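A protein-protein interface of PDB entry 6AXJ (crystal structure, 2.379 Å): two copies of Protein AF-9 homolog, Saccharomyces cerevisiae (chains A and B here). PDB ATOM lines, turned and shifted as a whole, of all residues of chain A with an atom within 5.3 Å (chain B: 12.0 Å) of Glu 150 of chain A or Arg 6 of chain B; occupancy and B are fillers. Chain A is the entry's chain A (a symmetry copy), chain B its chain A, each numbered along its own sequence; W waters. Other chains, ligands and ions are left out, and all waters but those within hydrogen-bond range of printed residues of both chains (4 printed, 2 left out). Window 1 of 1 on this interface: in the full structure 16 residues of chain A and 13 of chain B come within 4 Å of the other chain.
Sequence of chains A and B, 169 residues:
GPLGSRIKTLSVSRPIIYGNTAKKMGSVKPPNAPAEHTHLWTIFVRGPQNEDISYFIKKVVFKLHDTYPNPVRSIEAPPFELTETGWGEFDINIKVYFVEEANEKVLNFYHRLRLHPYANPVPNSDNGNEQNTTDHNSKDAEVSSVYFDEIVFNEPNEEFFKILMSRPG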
ATOM      1  N   SER A  13       9.958  -8.753  10.767  1.00  0.00           N
ATOM      2  CA  SER A  13      11.162  -7.969  10.556  1.00  0.00           C
ATOM      3  C   SER A  13      12.324  -8.519  11.380  1.00  0.00           C
ATOM      4  O   SER A  13      12.135  -9.035  12.482  1.00  0.00           O
ATOM      5  CB  SER A  13      10.910  -6.512  10.895  1.00  0.00           C
ATOM      6  OG  SER A  13      10.508  -6.371  12.233  1.00  0.00           O
ATOM      7  N   ARG A  14      13.533  -8.410  10.824  1.00  0.00           N
ATOM      8  CA  ARG A  14      14.754  -8.897  11.468  1.00  0.00           C
ATOM      9  C   ARG A  14      15.787  -7.782  11.417  1.00  0.00           C
ATOM     10  O   ARG A  14      16.173  -7.352  10.312  1.00  0.00           O
ATOM     11  CB  ARG A  14      15.295 -10.165  10.796  1.00  0.00           C
ATOM     12  CG  ARG A  14      14.603 -11.429  11.227  1.00  0.00           C
ATOM     13  CD  ARG A  14      14.676 -11.555  12.724  1.00  0.00           C
ATOM     14  NE  ARG A  14      13.915 -12.693  13.209  1.00  0.00           N
ATOM     15  CZ  ARG A  14      12.732 -12.600  13.810  1.00  0.00           C
ATOM     16  NH1 ARG A  14      12.167 -11.417  14.006  1.00  0.00           N
ATOM     17  NH2 ARG A  14      12.112 -13.693  14.210  1.00  0.00           N
ATOM     18  N   PRO A  15      16.247  -7.277  12.564  1.00  0.00           N
ATOM     19  CA  PRO A  15      17.260  -6.213  12.557  1.00  0.00           C
ATOM     20  C   PRO A  15      18.550  -6.704  11.934  1.00  0.00           C
ATOM     21  O   PRO A  15      18.927  -7.870  12.072  1.00  0.00           O
ATOM     22  CB  PRO A  15      17.462  -5.894  14.042  1.00  0.00           C
ATOM     23  CG  PRO A  15      16.280  -6.490  14.739  1.00  0.00           C
ATOM     24  CD  PRO A  15      15.879  -7.679  13.930  1.00  0.00           C
ATOM     25  N   ILE A  16      19.240  -5.794  11.255  1.00  0.00           N
ATOM     26  CA  ILE A  16      20.432  -6.162  10.507  1.00  0.00           C
ATOM     27  C   ILE A  16      21.424  -5.008  10.574  1.00  0.00           C
ATOM     28  O   ILE A  16      21.046  -3.838  10.455  1.00  0.00           O
ATOM     29  CB  ILE A  16      20.063  -6.542   9.055  1.00  0.00           C
ATOM     30  CG1 ILE A  16      21.054  -7.561   8.495  1.00  0.00           C
ATOM     31  CG2 ILE A  16      19.875  -5.306   8.159  1.00  0.00           C
ATOM     32  CD1 ILE A  16      20.890  -8.935   9.125  1.00  0.00           C
ATOM     33  N   LEU A 107      18.042 -10.313  -1.643  1.00  0.00           N
ATOM     34  CA  LEU A 107      17.931  -8.963  -1.104  1.00  0.00           C
ATOM     35  C   LEU A 107      19.155  -8.172  -1.568  1.00  0.00           C
ATOM     36  O   LEU A 107      20.295  -8.523  -1.246  1.00  0.00           O
ATOM     37  CB  LEU A 107      17.803  -8.971   0.420  1.00  0.00           C
ATOM     38  CG  LEU A 107      17.753  -7.616   1.133  1.00  0.00           C
ATOM     39  CD1 LEU A 107      16.590  -6.758   0.634  1.00  0.00           C
ATOM     40  CD2 LEU A 107      17.668  -7.810   2.646  1.00  0.00           C
ATOM     41  N   PHE A 148      22.274   0.281  10.872  1.00  0.00           N
ATOM     42  CA  PHE A 148      21.558  -0.611  11.779  1.00  0.00           C
ATOM     43  C   PHE A 148      20.084  -0.466  11.396  1.00  0.00           C
ATOM     44  O   PHE A 148      19.350   0.344  11.968  1.00  0.00           O
ATOM     45  CB  PHE A 148      21.828  -0.244  13.256  1.00  0.00           C
ATOM     46  CG  PHE A 148      21.168  -1.173  14.281  1.00  0.00           C
ATOM     47  CD1 PHE A 148      20.672  -2.407  13.923  1.00  0.00           C
ATOM     48  CD2 PHE A 148      21.056  -0.782  15.610  1.00  0.00           C
ATOM     49  CE1 PHE A 148      20.088  -3.244  14.869  1.00  0.00           C
ATOM     50  CE2 PHE A 148      20.465  -1.609  16.567  1.00  0.00           C
ATOM     51  CZ  PHE A 148      19.985  -2.848  16.194  1.00  0.00           C
ATOM     52  N   ASP A 149      19.671  -1.251  10.400  1.00  0.00           N
ATOM     53  CA  ASP A 149      18.312  -1.228   9.882  1.00  0.00           C
ATOM     54  C   ASP A 149      17.629  -2.552  10.185  1.00  0.00           C
ATOM     55  O   ASP A 149      18.036  -3.279  11.102  1.00  0.00           O
ATOM     56  CB  ASP A 149      18.316  -0.980   8.370  1.00  0.00           C
ATOM     57  CG  ASP A 149      19.009   0.311   7.995  1.00  0.00           C
ATOM     58  OD1 ASP A 149      18.867   1.294   8.748  1.00  0.00           O
ATOM     59  OD2 ASP A 149      19.679   0.350   6.940  1.00  0.00           O
ATOM     60  N   GLU A 150      16.623  -2.904   9.388  1.00  0.00           N
ATOM     61  CA  GLU A 150      15.919  -4.157   9.594  1.00  0.00           C
ATOM     62  C   GLU A 150      15.442  -4.666   8.249  1.00  0.00           C
ATOM     63  O   GLU A 150      15.209  -3.891   7.320  1.00  0.00           O
ATOM     64  CB  GLU A 150      14.748  -3.983  10.572  1.00  0.00           C
ATOM     65  CG  GLU A 150      13.505  -3.366   9.981  1.00  0.00           C
ATOM     66  CD  GLU A 150      12.460  -3.007  11.040  1.00  0.00           C
ATOM     67  OE1 GLU A 150      12.656  -3.255  12.242  1.00  0.00           O
ATOM     68  OE2 GLU A 150      11.394  -2.525  10.658  1.00  0.00           O
ATOM     69  N   ILE A 151      15.375  -5.981   8.127  1.00  0.00           N
ATOM     70  CA  ILE A 151      14.837  -6.630   6.941  1.00  0.00           C
ATOM     71  C   ILE A 151      13.387  -6.964   7.240  1.00  0.00           C
ATOM     72  O   ILE A 151      13.106  -7.651   8.229  1.00  0.00           O
ATOM     73  CB  ILE A 151      15.626  -7.898   6.587  1.00  0.00           C
ATOM     74  CG1 ILE A 151      17.109  -7.587   6.349  1.00  0.00           C
ATOM     75  CG2 ILE A 151      15.011  -8.616   5.393  1.00  0.00           C
ATOM     76  CD1 ILE A 151      17.935  -8.841   6.104  1.00  0.00           C
ATOM     77  N   VAL A 152      12.467  -6.489   6.409  1.00  0.00           N
ATOM     78  CA  VAL A 152      11.058  -6.825   6.561  1.00  0.00           C
ATOM     79  C   VAL A 152      10.738  -7.963   5.607  1.00  0.00           C
ATOM     80  O   VAL A 152      11.008  -7.872   4.405  1.00  0.00           O
ATOM     81  CB  VAL A 152      10.147  -5.617   6.308  1.00  0.00           C
ATOM     82  CG1 VAL A 152       8.718  -5.996   6.590  1.00  0.00           C
ATOM     83  CG2 VAL A 152      10.543  -4.487   7.194  1.00  0.00           C
ATOM     84  N   ASN A 154       7.807  -9.851   3.878  1.00  0.00           N
ATOM     85  CA  ASN A 154       6.411  -9.735   3.481  1.00  0.00           C
ATOM     86  C   ASN A 154       5.825 -11.128   3.246  1.00  0.00           C
ATOM     87  O   ASN A 154       6.425 -11.932   2.529  1.00  0.00           O
ATOM     88  CB  ASN A 154       6.368  -8.938   2.175  1.00  0.00           C
ATOM     89  CG  ASN A 154       5.240  -7.978   2.114  1.00  0.00           C
ATOM     90  OD1 ASN A 154       5.104  -7.117   2.976  1.00  0.00           O
ATOM     91  ND2 ASN A 154       4.406  -8.110   1.085  1.00  0.00           N
ATOM     92  N   GLY B   4       8.249 -11.565   0.041  1.00  0.00           N
ATOM     93  CA  GLY B   4       9.216 -10.549  -0.344  1.00  0.00           C
ATOM     94  C   GLY B   4      10.038  -9.998   0.811  1.00  0.00           C
ATOM     95  O   GLY B   4       9.677 -10.169   1.972  1.00  0.00           O
ATOM     96  N   SER B   5      11.143  -9.321   0.499  1.00  0.00           N
ATOM     97  CA  SER B   5      11.977  -8.728   1.537  1.00  0.00           C
ATOM     98  C   SER B   5      12.428  -7.336   1.125  1.00  0.00           C
ATOM     99  O   SER B   5      12.696  -7.079  -0.053  1.00  0.00           O
ATOM    100  CB  SER B   5      13.206  -9.599   1.845  1.00  0.00           C
ATOM    101  OG  SER B   5      14.116  -9.591   0.765  1.00  0.00           O
ATOM    102  N   ARG B   6      12.518  -6.443   2.103  1.00  0.00           N
ATOM    103  CA  ARG B   6      13.029  -5.109   1.853  1.00  0.00           C
ATOM    104  C   ARG B   6      13.735  -4.625   3.108  1.00  0.00           C
ATOM    105  O   ARG B   6      13.498  -5.121   4.212  1.00  0.00           O
ATOM    106  CB  ARG B   6      11.909  -4.138   1.464  1.00  0.00           C
ATOM    107  CG  ARG B   6      10.947  -3.849   2.600  1.00  0.00           C
ATOM    108  CD  ARG B   6       9.846  -2.873   2.179  1.00  0.00           C
ATOM    109  NE  ARG B   6       8.913  -2.547   3.265  1.00  0.00           N
ATOM    110  CZ  ARG B   6       7.855  -3.290   3.590  1.00  0.00           C
ATOM    111  NH1 ARG B   6       7.590  -4.411   2.931  1.00  0.00           N
ATOM    112  NH2 ARG B   6       7.056  -2.913   4.580  1.00  0.00           N
ATOM    113  N   ILE B   7      14.602  -3.641   2.924  1.00  0.00           N
ATOM    114  CA  ILE B   7      15.261  -2.962   4.033  1.00  0.00           C
ATOM    115  C   ILE B   7      14.456  -1.717   4.383  1.00  0.00           C
ATOM    116  O   ILE B   7      14.050  -0.956   3.499  1.00  0.00           O
ATOM    117  CB  ILE B   7      16.717  -2.609   3.681  1.00  0.00           C
ATOM    118  CG1 ILE B   7      17.546  -3.888   3.534  1.00  0.00           C
ATOM    119  CG2 ILE B   7      17.299  -1.648   4.721  1.00  0.00           C
ATOM    120  CD1 ILE B   7      19.019  -3.651   3.292  1.00  0.00           C
ATOM    121  N   LYS B   8      14.195  -1.528   5.667  1.00  0.00           N
ATOM    122  CA  LYS B   8      13.554  -0.321   6.154  1.00  0.00           C
ATOM    123  C   LYS B   8      14.271   0.124   7.419  1.00  0.00           C
ATOM    124  O   LYS B   8      15.118  -0.590   7.967  1.00  0.00           O
ATOM    125  CB  LYS B   8      12.057  -0.550   6.420  1.00  0.00           C
ATOM    126  CG  LYS B   8      11.785  -1.161   7.761  1.00  0.00           C
ATOM    127  CD  LYS B   8      10.315  -1.163   8.144  1.00  0.00           C
ATOM    128  CE  LYS B   8       9.698   0.210   8.283  1.00  0.00           C
ATOM    129  NZ  LYS B   8       8.213   0.038   8.331  1.00  0.00           N
ATOM    130  N   THR B   9      13.936   1.321   7.887  1.00  0.00           N
ATOM    131  CA  THR B   9      14.577   1.809   9.094  1.00  0.00           C
ATOM    132  C   THR B   9      14.073   1.019  10.296  1.00  0.00           C
ATOM    133  O   THR B   9      12.911   0.594  10.353  1.00  0.00           O
ATOM    134  CB  THR B   9      14.343   3.314   9.285  1.00  0.00           C
ATOM    135  OG1 THR B   9      12.965   3.568   9.565  1.00  0.00           O
ATOM    136  CG2 THR B   9      14.751   4.073   8.043  1.00  0.00           C
ATOM    137  N   LEU B  10      14.972   0.786  11.237  1.00  0.00           N
ATOM    138  CA  LEU B  10      14.647   0.014  12.416  1.00  0.00           C
ATOM    139  C   LEU B  10      13.877   0.877  13.402  1.00  0.00           C
ATOM    140  O   LEU B  10      14.227   2.039  13.642  1.00  0.00           O
ATOM    141  CB  LEU B  10      15.929  -0.528  13.055  1.00  0.00           C
ATOM    142  CG  LEU B  10      15.773  -1.166  14.433  1.00  0.00           C
ATOM    143  CD1 LEU B  10      15.008  -2.466  14.358  1.00  0.00           C
ATOM    144  CD2 LEU B  10      17.133  -1.379  15.076  1.00  0.00           C
ATOM    145  N   SER B  11      12.838   0.294  13.987  1.00  0.00           N
ATOM    146  CA  SER B  11      12.109   0.924  15.067  1.00  0.00           C
ATOM    147  C   SER B  11      11.754  -0.133  16.100  1.00  0.00           C
ATOM    148  O   SER B  11      11.592  -1.309  15.774  1.00  0.00           O
ATOM    149  CB  SER B  11      10.855   1.634  14.541  1.00  0.00           C
ATOM    150  OG  SER B  11       9.798   0.723  14.333  1.00  0.00           O
ATOM    151  N   VAL B  12      11.687   0.286  17.360  1.00  0.00           N
ATOM    152  CA  VAL B  12      11.274  -0.572  18.464  1.00  0.00           C
ATOM    153  C   VAL B  12      10.280   0.191  19.325  1.00  0.00           C
ATOM    154  O   VAL B  12      10.501   1.361  19.658  1.00  0.00           O
ATOM    155  CB  VAL B  12      12.475  -1.035  19.312  1.00  0.00           C
ATOM    156  CG1 VAL B  12      11.996  -1.805  20.527  1.00  0.00           C
ATOM    157  CG2 VAL B  12      13.425  -1.867  18.471  1.00  0.00           C
ATOM    158  N   SER B  13       9.204  -0.476  19.711  1.00  0.00           N
ATOM    159  CA  SER B  13       8.145   0.155  20.478  1.00  0.00           C
ATOM    160  C   SER B  13       8.032  -0.466  21.869  1.00  0.00           C
ATOM    161  O   SER B  13       8.271  -1.660  22.054  1.00  0.00           O
ATOM    162  CB  SER B  13       6.823   0.052  19.740  1.00  0.00           C
ATOM    163  OG  SER B  13       6.479  -1.291  19.513  1.00  0.00           O
ATOM    164  N   ARG B  14       7.673   0.367  22.849  1.00  0.00           N
ATOM    165  CA  ARG B  14       7.531  -0.056  24.242  1.00  0.00           C
ATOM    166  C   ARG B  14       6.188   0.446  24.750  1.00  0.00           C
ATOM    167  O   ARG B  14       5.961   1.672  24.777  1.00  0.00           O
ATOM    168  CB  ARG B  14       8.672   0.467  25.123  1.00  0.00           C
ATOM    169  CG  ARG B  14       9.933  -0.347  25.040  1.00  0.00           C
ATOM    170  CD  ARG B  14       9.628  -1.781  25.374  1.00  0.00           C
ATOM    171  NE  ARG B  14      10.785  -2.639  25.185  1.00  0.00           N
ATOM    172  CZ  ARG B  14      10.941  -3.468  24.158  1.00  0.00           C
ATOM    173  NH1 ARG B  14      10.011  -3.561  23.218  1.00  0.00           N
ATOM    174  NH2 ARG B  14      12.032  -4.205  24.069  1.00  0.00           N
ATOM    175  N   VAL B 152       7.461   4.696  20.497  1.00  0.00           N
ATOM    176  CA  VAL B 152       8.200   4.158  19.362  1.00  0.00           C
ATOM    177  C   VAL B 152       9.588   4.776  19.367  1.00  0.00           C
ATOM    178  O   VAL B 152       9.732   6.002  19.404  1.00  0.00           O
ATOM    179  CB  VAL B 152       7.482   4.420  18.032  1.00  0.00           C
ATOM    180  CG1 VAL B 152       8.232   3.745  16.914  1.00  0.00           C
ATOM    181  CG2 VAL B 152       6.094   3.884  18.090  1.00  0.00           C
ATOM    182  N   PHE B 153      10.611   3.935  19.368  1.00  0.00           N
ATOM    183  CA  PHE B 153      11.987   4.389  19.232  1.00  0.00           C
ATOM    184  C   PHE B 153      12.423   4.245  17.780  1.00  0.00           C
ATOM    185  O   PHE B 153      12.472   3.131  17.240  1.00  0.00           O
ATOM    186  CB  PHE B 153      12.914   3.645  20.189  1.00  0.00           C
ATOM    187  CG  PHE B 153      12.609   3.912  21.636  1.00  0.00           C
ATOM    188  CD1 PHE B 153      12.963   5.126  22.212  1.00  0.00           C
ATOM    189  CD2 PHE B 153      11.952   2.967  22.419  1.00  0.00           C
ATOM    190  CE1 PHE B 153      12.688   5.389  23.557  1.00  0.00           C
ATOM    191  CE2 PHE B 153      11.666   3.231  23.763  1.00  0.00           C
ATOM    192  CZ  PHE B 153      12.039   4.441  24.334  1.00  0.00           C
ATOM    193  N   ASN B 154      12.738   5.381  17.165  1.00  0.00           N
ATOM    194  CA  ASN B 154      13.210   5.457  15.789  1.00  0.00           C
ATOM    195  C   ASN B 154      14.728   5.277  15.754  1.00  0.00           C
ATOM    196  O   ASN B 154      15.442   5.946  16.505  1.00  0.00           O
ATOM    197  CB  ASN B 154      12.848   6.844  15.254  1.00  0.00           C
ATOM    198  CG  ASN B 154      12.377   6.824  13.850  1.00  0.00           C
ATOM    199  OD1 ASN B 154      11.418   6.135  13.521  1.00  0.00           O
ATOM    200  ND2 ASN B 154      13.049   7.586  12.989  1.00  0.00           N
ATOM    201  N   GLU B 155      15.225   4.393  14.869  1.00  0.00           N
ATOM    202  CA  GLU B 155      16.660   4.148  14.658  1.00  0.00           C
ATOM    203  C   GLU B 155      17.486   4.038  15.941  1.00  0.00           C
ATOM    204  O   GLU B 155      18.494   4.740  16.074  1.00  0.00           O
ATOM    205  CB  GLU B 155      17.268   5.255  13.793  1.00  0.00           C
ATOM    206  CG  GLU B 155      16.490   5.511  12.516  1.00  0.00           C
ATOM    207  CD  GLU B 155      17.179   6.489  11.590  1.00  0.00           C
ATOM    208  OE1 GLU B 155      18.386   6.738  11.775  1.00  0.00           O
ATOM    209  OE2 GLU B 155      16.514   6.998  10.667  1.00  0.00           O
ATOM    210  N   PRO B 156      17.128   3.178  16.892  1.00  0.00           N
ATOM    211  CA  PRO B 156      17.926   3.082  18.119  1.00  0.00           C
ATOM    212  C   PRO B 156      19.323   2.559  17.822  1.00  0.00           C
ATOM    213  O   PRO B 156      19.528   1.753  16.910  1.00  0.00           O
ATOM    214  CB  PRO B 156      17.128   2.099  18.975  1.00  0.00           C
ATOM    215  CG  PRO B 156      16.546   1.179  17.945  1.00  0.00           C
ATOM    216  CD  PRO B 156      16.164   2.070  16.790  1.00  0.00           C
ATOM    217  N   ASN B 157      20.295   3.030  18.602  1.00  0.00           N
ATOM    218  CA  ASN B 157      21.655   2.558  18.405  1.00  0.00           C
ATOM    219  C   ASN B 157      21.788   1.151  18.976  1.00  0.00           C
ATOM    220  O   ASN B 157      20.937   0.685  19.741  1.00  0.00           O
ATOM    221  CB  ASN B 157      22.684   3.530  19.029  1.00  0.00           C
ATOM    222  CG  ASN B 157      22.559   3.657  20.559  1.00  0.00           C
ATOM    223  OD1 ASN B 157      22.820   2.707  21.312  1.00  0.00           O
ATOM    224  ND2 ASN B 157      22.172   4.839  21.015  1.00  0.00           N
ATOM    225  N   GLU B 158      22.869   0.468  18.589  1.00  0.00           N
ATOM    226  CA  GLU B 158      22.990  -0.948  18.928  1.00  0.00           C
ATOM    227  C   GLU B 158      22.970  -1.177  20.438  1.00  0.00           C
ATOM    228  O   GLU B 158      22.339  -2.129  20.913  1.00  0.00           O
ATOM    229  CB  GLU B 158      24.259  -1.538  18.315  1.00  0.00           C
ATOM    230  CG  GLU B 158      24.369  -3.063  18.502  1.00  0.00           C
ATOM    231  CD  GLU B 158      25.520  -3.655  17.718  1.00  0.00           C
ATOM    232  OE1 GLU B 158      26.309  -2.866  17.158  1.00  0.00           O
ATOM    233  OE2 GLU B 158      25.622  -4.897  17.619  1.00  0.00           O
ATOM    234  N   PHE B 161      19.393  -0.728  21.696  1.00  0.00           N
ATOM    235  CA  PHE B 161      18.600  -1.865  21.252  1.00  0.00           C
ATOM    236  C   PHE B 161      18.853  -3.084  22.133  1.00  0.00           C
ATOM    237  O   PHE B 161      17.925  -3.844  22.439  1.00  0.00           O
ATOM    238  CB  PHE B 161      18.925  -2.156  19.791  1.00  0.00           C
ATOM    239  CG  PHE B 161      18.244  -3.355  19.241  1.00  0.00           C
ATOM    240  CD1 PHE B 161      17.002  -3.243  18.640  1.00  0.00           C
ATOM    241  CD2 PHE B 161      18.855  -4.601  19.293  1.00  0.00           C
ATOM    242  CE1 PHE B 161      16.369  -4.362  18.096  1.00  0.00           C
ATOM    243  CE2 PHE B 161      18.228  -5.716  18.770  1.00  0.00           C
ATOM    244  CZ  PHE B 161      16.980  -5.596  18.162  1.00  0.00           C
ATOM    245  N   LEU B 164      16.919  -2.452  25.218  1.00  0.00           N
ATOM    246  CA  LEU B 164      15.474  -2.560  25.019  1.00  0.00           C
ATOM    247  C   LEU B 164      15.034  -4.010  24.911  1.00  0.00           C
ATOM    248  O   LEU B 164      13.933  -4.357  25.350  1.00  0.00           O
ATOM    249  CB  LEU B 164      15.033  -1.793  23.772  1.00  0.00           C
ATOM    250  CG  LEU B 164      14.987  -0.263  23.775  1.00  0.00           C
ATOM    251  CD1 LEU B 164      14.819   0.260  22.332  1.00  0.00           C
ATOM    252  CD2 LEU B 164      13.877   0.270  24.684  1.00  0.00           C
ATOM    253  N   MET B 165      15.874  -4.862  24.332  1.00  0.00           N
ATOM    254  CA  MET B 165      15.538  -6.263  24.133  1.00  0.00           C
ATOM    255  C   MET B 165      15.770  -7.116  25.371  1.00  0.00           C
ATOM    256  O   MET B 165      15.344  -8.275  25.389  1.00  0.00           O
ATOM    257  CB  MET B 165      16.338  -6.824  22.953  1.00  0.00           C
ATOM    258  CG  MET B 165      15.941  -6.243  21.605  1.00  0.00           C
ATOM    259  SD  MET B 165      14.181  -6.490  21.284  1.00  0.00           S
ATOM    260  CE  MET B 165      13.660  -4.848  20.878  1.00  0.00           C
HETATM  261  O   HOH W   1       8.891  -6.893   2.479  1.00  0.00           O
HETATM  262  O   HOH W   2       9.915  -0.472  11.647  1.00  0.00           O
HETATM  263  O   HOH W   3      17.594   2.330  11.185  1.00  0.00           O
HETATM  264  O   HOH W   4       9.754  -2.679  13.504  1.00  0.00           O
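The backbone carbonyl oxygen (O) of Gly 4 of chain B sits at hydrogen-bond distance from the backbone NH (N) of Asn 154 of chain A (2.7 Å).
O of Glu 150 of chain A sits at hydrogen-bond distance from N of Lys 8 of chain B, 3.1 Å away.
The backbone carbonyl oxygen (O) of Thr 9 of chain B sits close to the side-chain carboxylate (OE2) of Glu 150 of chain A (3.5 Å).
The backbone carbonyl oxygen (O) of Arg 6 of chain B is in hydrogen-bond range of the backbone NH (N) of Val 152 of chain A (2.8 Å).
The backbone carbonyl oxygen (O) of Asp 149 of chain A is in hydrogen-bond range of the backbone NH (N) of Ile 16 of chain A, 2.8 Å away.
The backbone carbonyl oxygen (O) of Arg 14 of chain A sits at hydrogen-bond distance from the backbone NH (N) of Ile 151 of chain A.
The backbone carbonyl oxygen (O) of Leu 10 of chain B is in hydrogen-bond range of the backbone NH (N) of Glu 155 of chain B (2.8 Å).
Pro 15 of chain A touches Phe 161 of chain B (CG to CZ, 3.6 Å).
CB of Leu 107 of chain A touches OG of Ser 5 of chain B, at 3.8 Å.
Phe 148 of chain A touches Pro 156 of chain B (CD2 to O, 3.2 Å).
Asn 157 of chain B touches Phe 148 of chain A.
Glu 158 of chain B touches Phe 148 of chain A (CA to CE2, 3.5 Å).
Lys 8 of chain B touches Asp 149 of chain A (O to CB, 3.2 Å).
Glu 150 of chain A touches Ile 7 of chain B.
Val 152 of chain A touches Ser 5 of chain B (O to CA, 3.1 Å).
Val 152 of chain A touches Lys 8 of chain B (CG2 to CD, 3.5 Å).
OD1 of Asn 154 of chain A touches NH1 of Arg 6 of chain B, 3.7 Å away.
Pro 15 of chain A touches just one residue of chain B: Phe 161 (3.6 Å).
No residue of chain B comes within 4 Å of Ile 16 of chain A.
Ile 151 of chain A touches just one residue of chain B: Arg 6 (3.4 Å).
Val 152 of chain A touches just these residues of chain B: Gly 4, Ser 5, Arg 6 and Lys 8.
Of chain B, only Gly 4 and Arg 6 come within 4 Å of Asn 154 of chain A.
Of the printed residues of chain A, Gly 4 of chain B touches Val 152 (3.6 Å) and Asn 154 (2.7 Å).
Arg 6 of chain B touches four residues of chain A.
Of the printed residues of chain A, Thr 9 of chain B touches Glu 150.
Printed residues of chain A within 4 Å of Leu 10 of chain B: Phe 148, Asp 149 and Glu 150.
Val 152 of chain B touches none of the printed residues of chain A.
Glu 155 of chain B touches none of the printed residues of chain A.
Printed residues of chain A within 4 Å of Pro 156 of chain B: Phe 148.
Of the printed residues of chain A, Asn 157 of chain B touches Phe 148 (3.9 Å).
The nearest residue of chain B that does not touch Glu 150 of chain A is Val 12 of chain B (6.3 Å).
The nearest printed residue of chain A that does not touch Ser 5 of chain B is Ile 151 of chain A (4.1 Å).
Of the 21 printed residues of chain B, 12 touch a printed residue of chain A.
Printed residues of chain B that touch a printed residue of chain A: Gly 4, Ser 5, Arg 6, Ile 7, Lys 8, Thr 9, Leu 10, Ser 11, Pro 156, Asn 157, Glu 158 and Phe 161.
Printed residues of chain A that touch a printed residue of chain B: Pro 15, Leu 107, Phe 148, Asp 149, Glu 150, Ile 151, Val 152 and Asn 154.
Hydrophobic or aromatic side chains of chain A that line the printed part of chain B: Pro 15, Leu 107, Phe 148, Ile 151 and Val 152.
Among the printed residues, 23 pairs touch across the chains.
4 positions are printed for both chains.
Water W2 lies within hydrogen-bond range of OE2 of Glu 150 of chain A (2.7 Å), OG of Ser 11 of chain B (2.9 Å) and O of Thr 9 of chain B (3.4 Å).
Water W3 lies within hydrogen-bond range of O of Phe 148 of chain A, OD1 of Asp 149 of chain A and N of Leu 10 of chain B.
Water W1 lies within hydrogen-bond range of NH1 of Arg 6 of chain B, O of Val 152 of chain A, O of Gly 4 of chain B and N of Asn 154 of chain A.
Water W4 bridges the side-chain carboxylate (OE1) of Glu 150 of chain A (3.2 Å) and the backbone carbonyl oxygen (O) of Ser 11 of chain B (3.2 Å).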
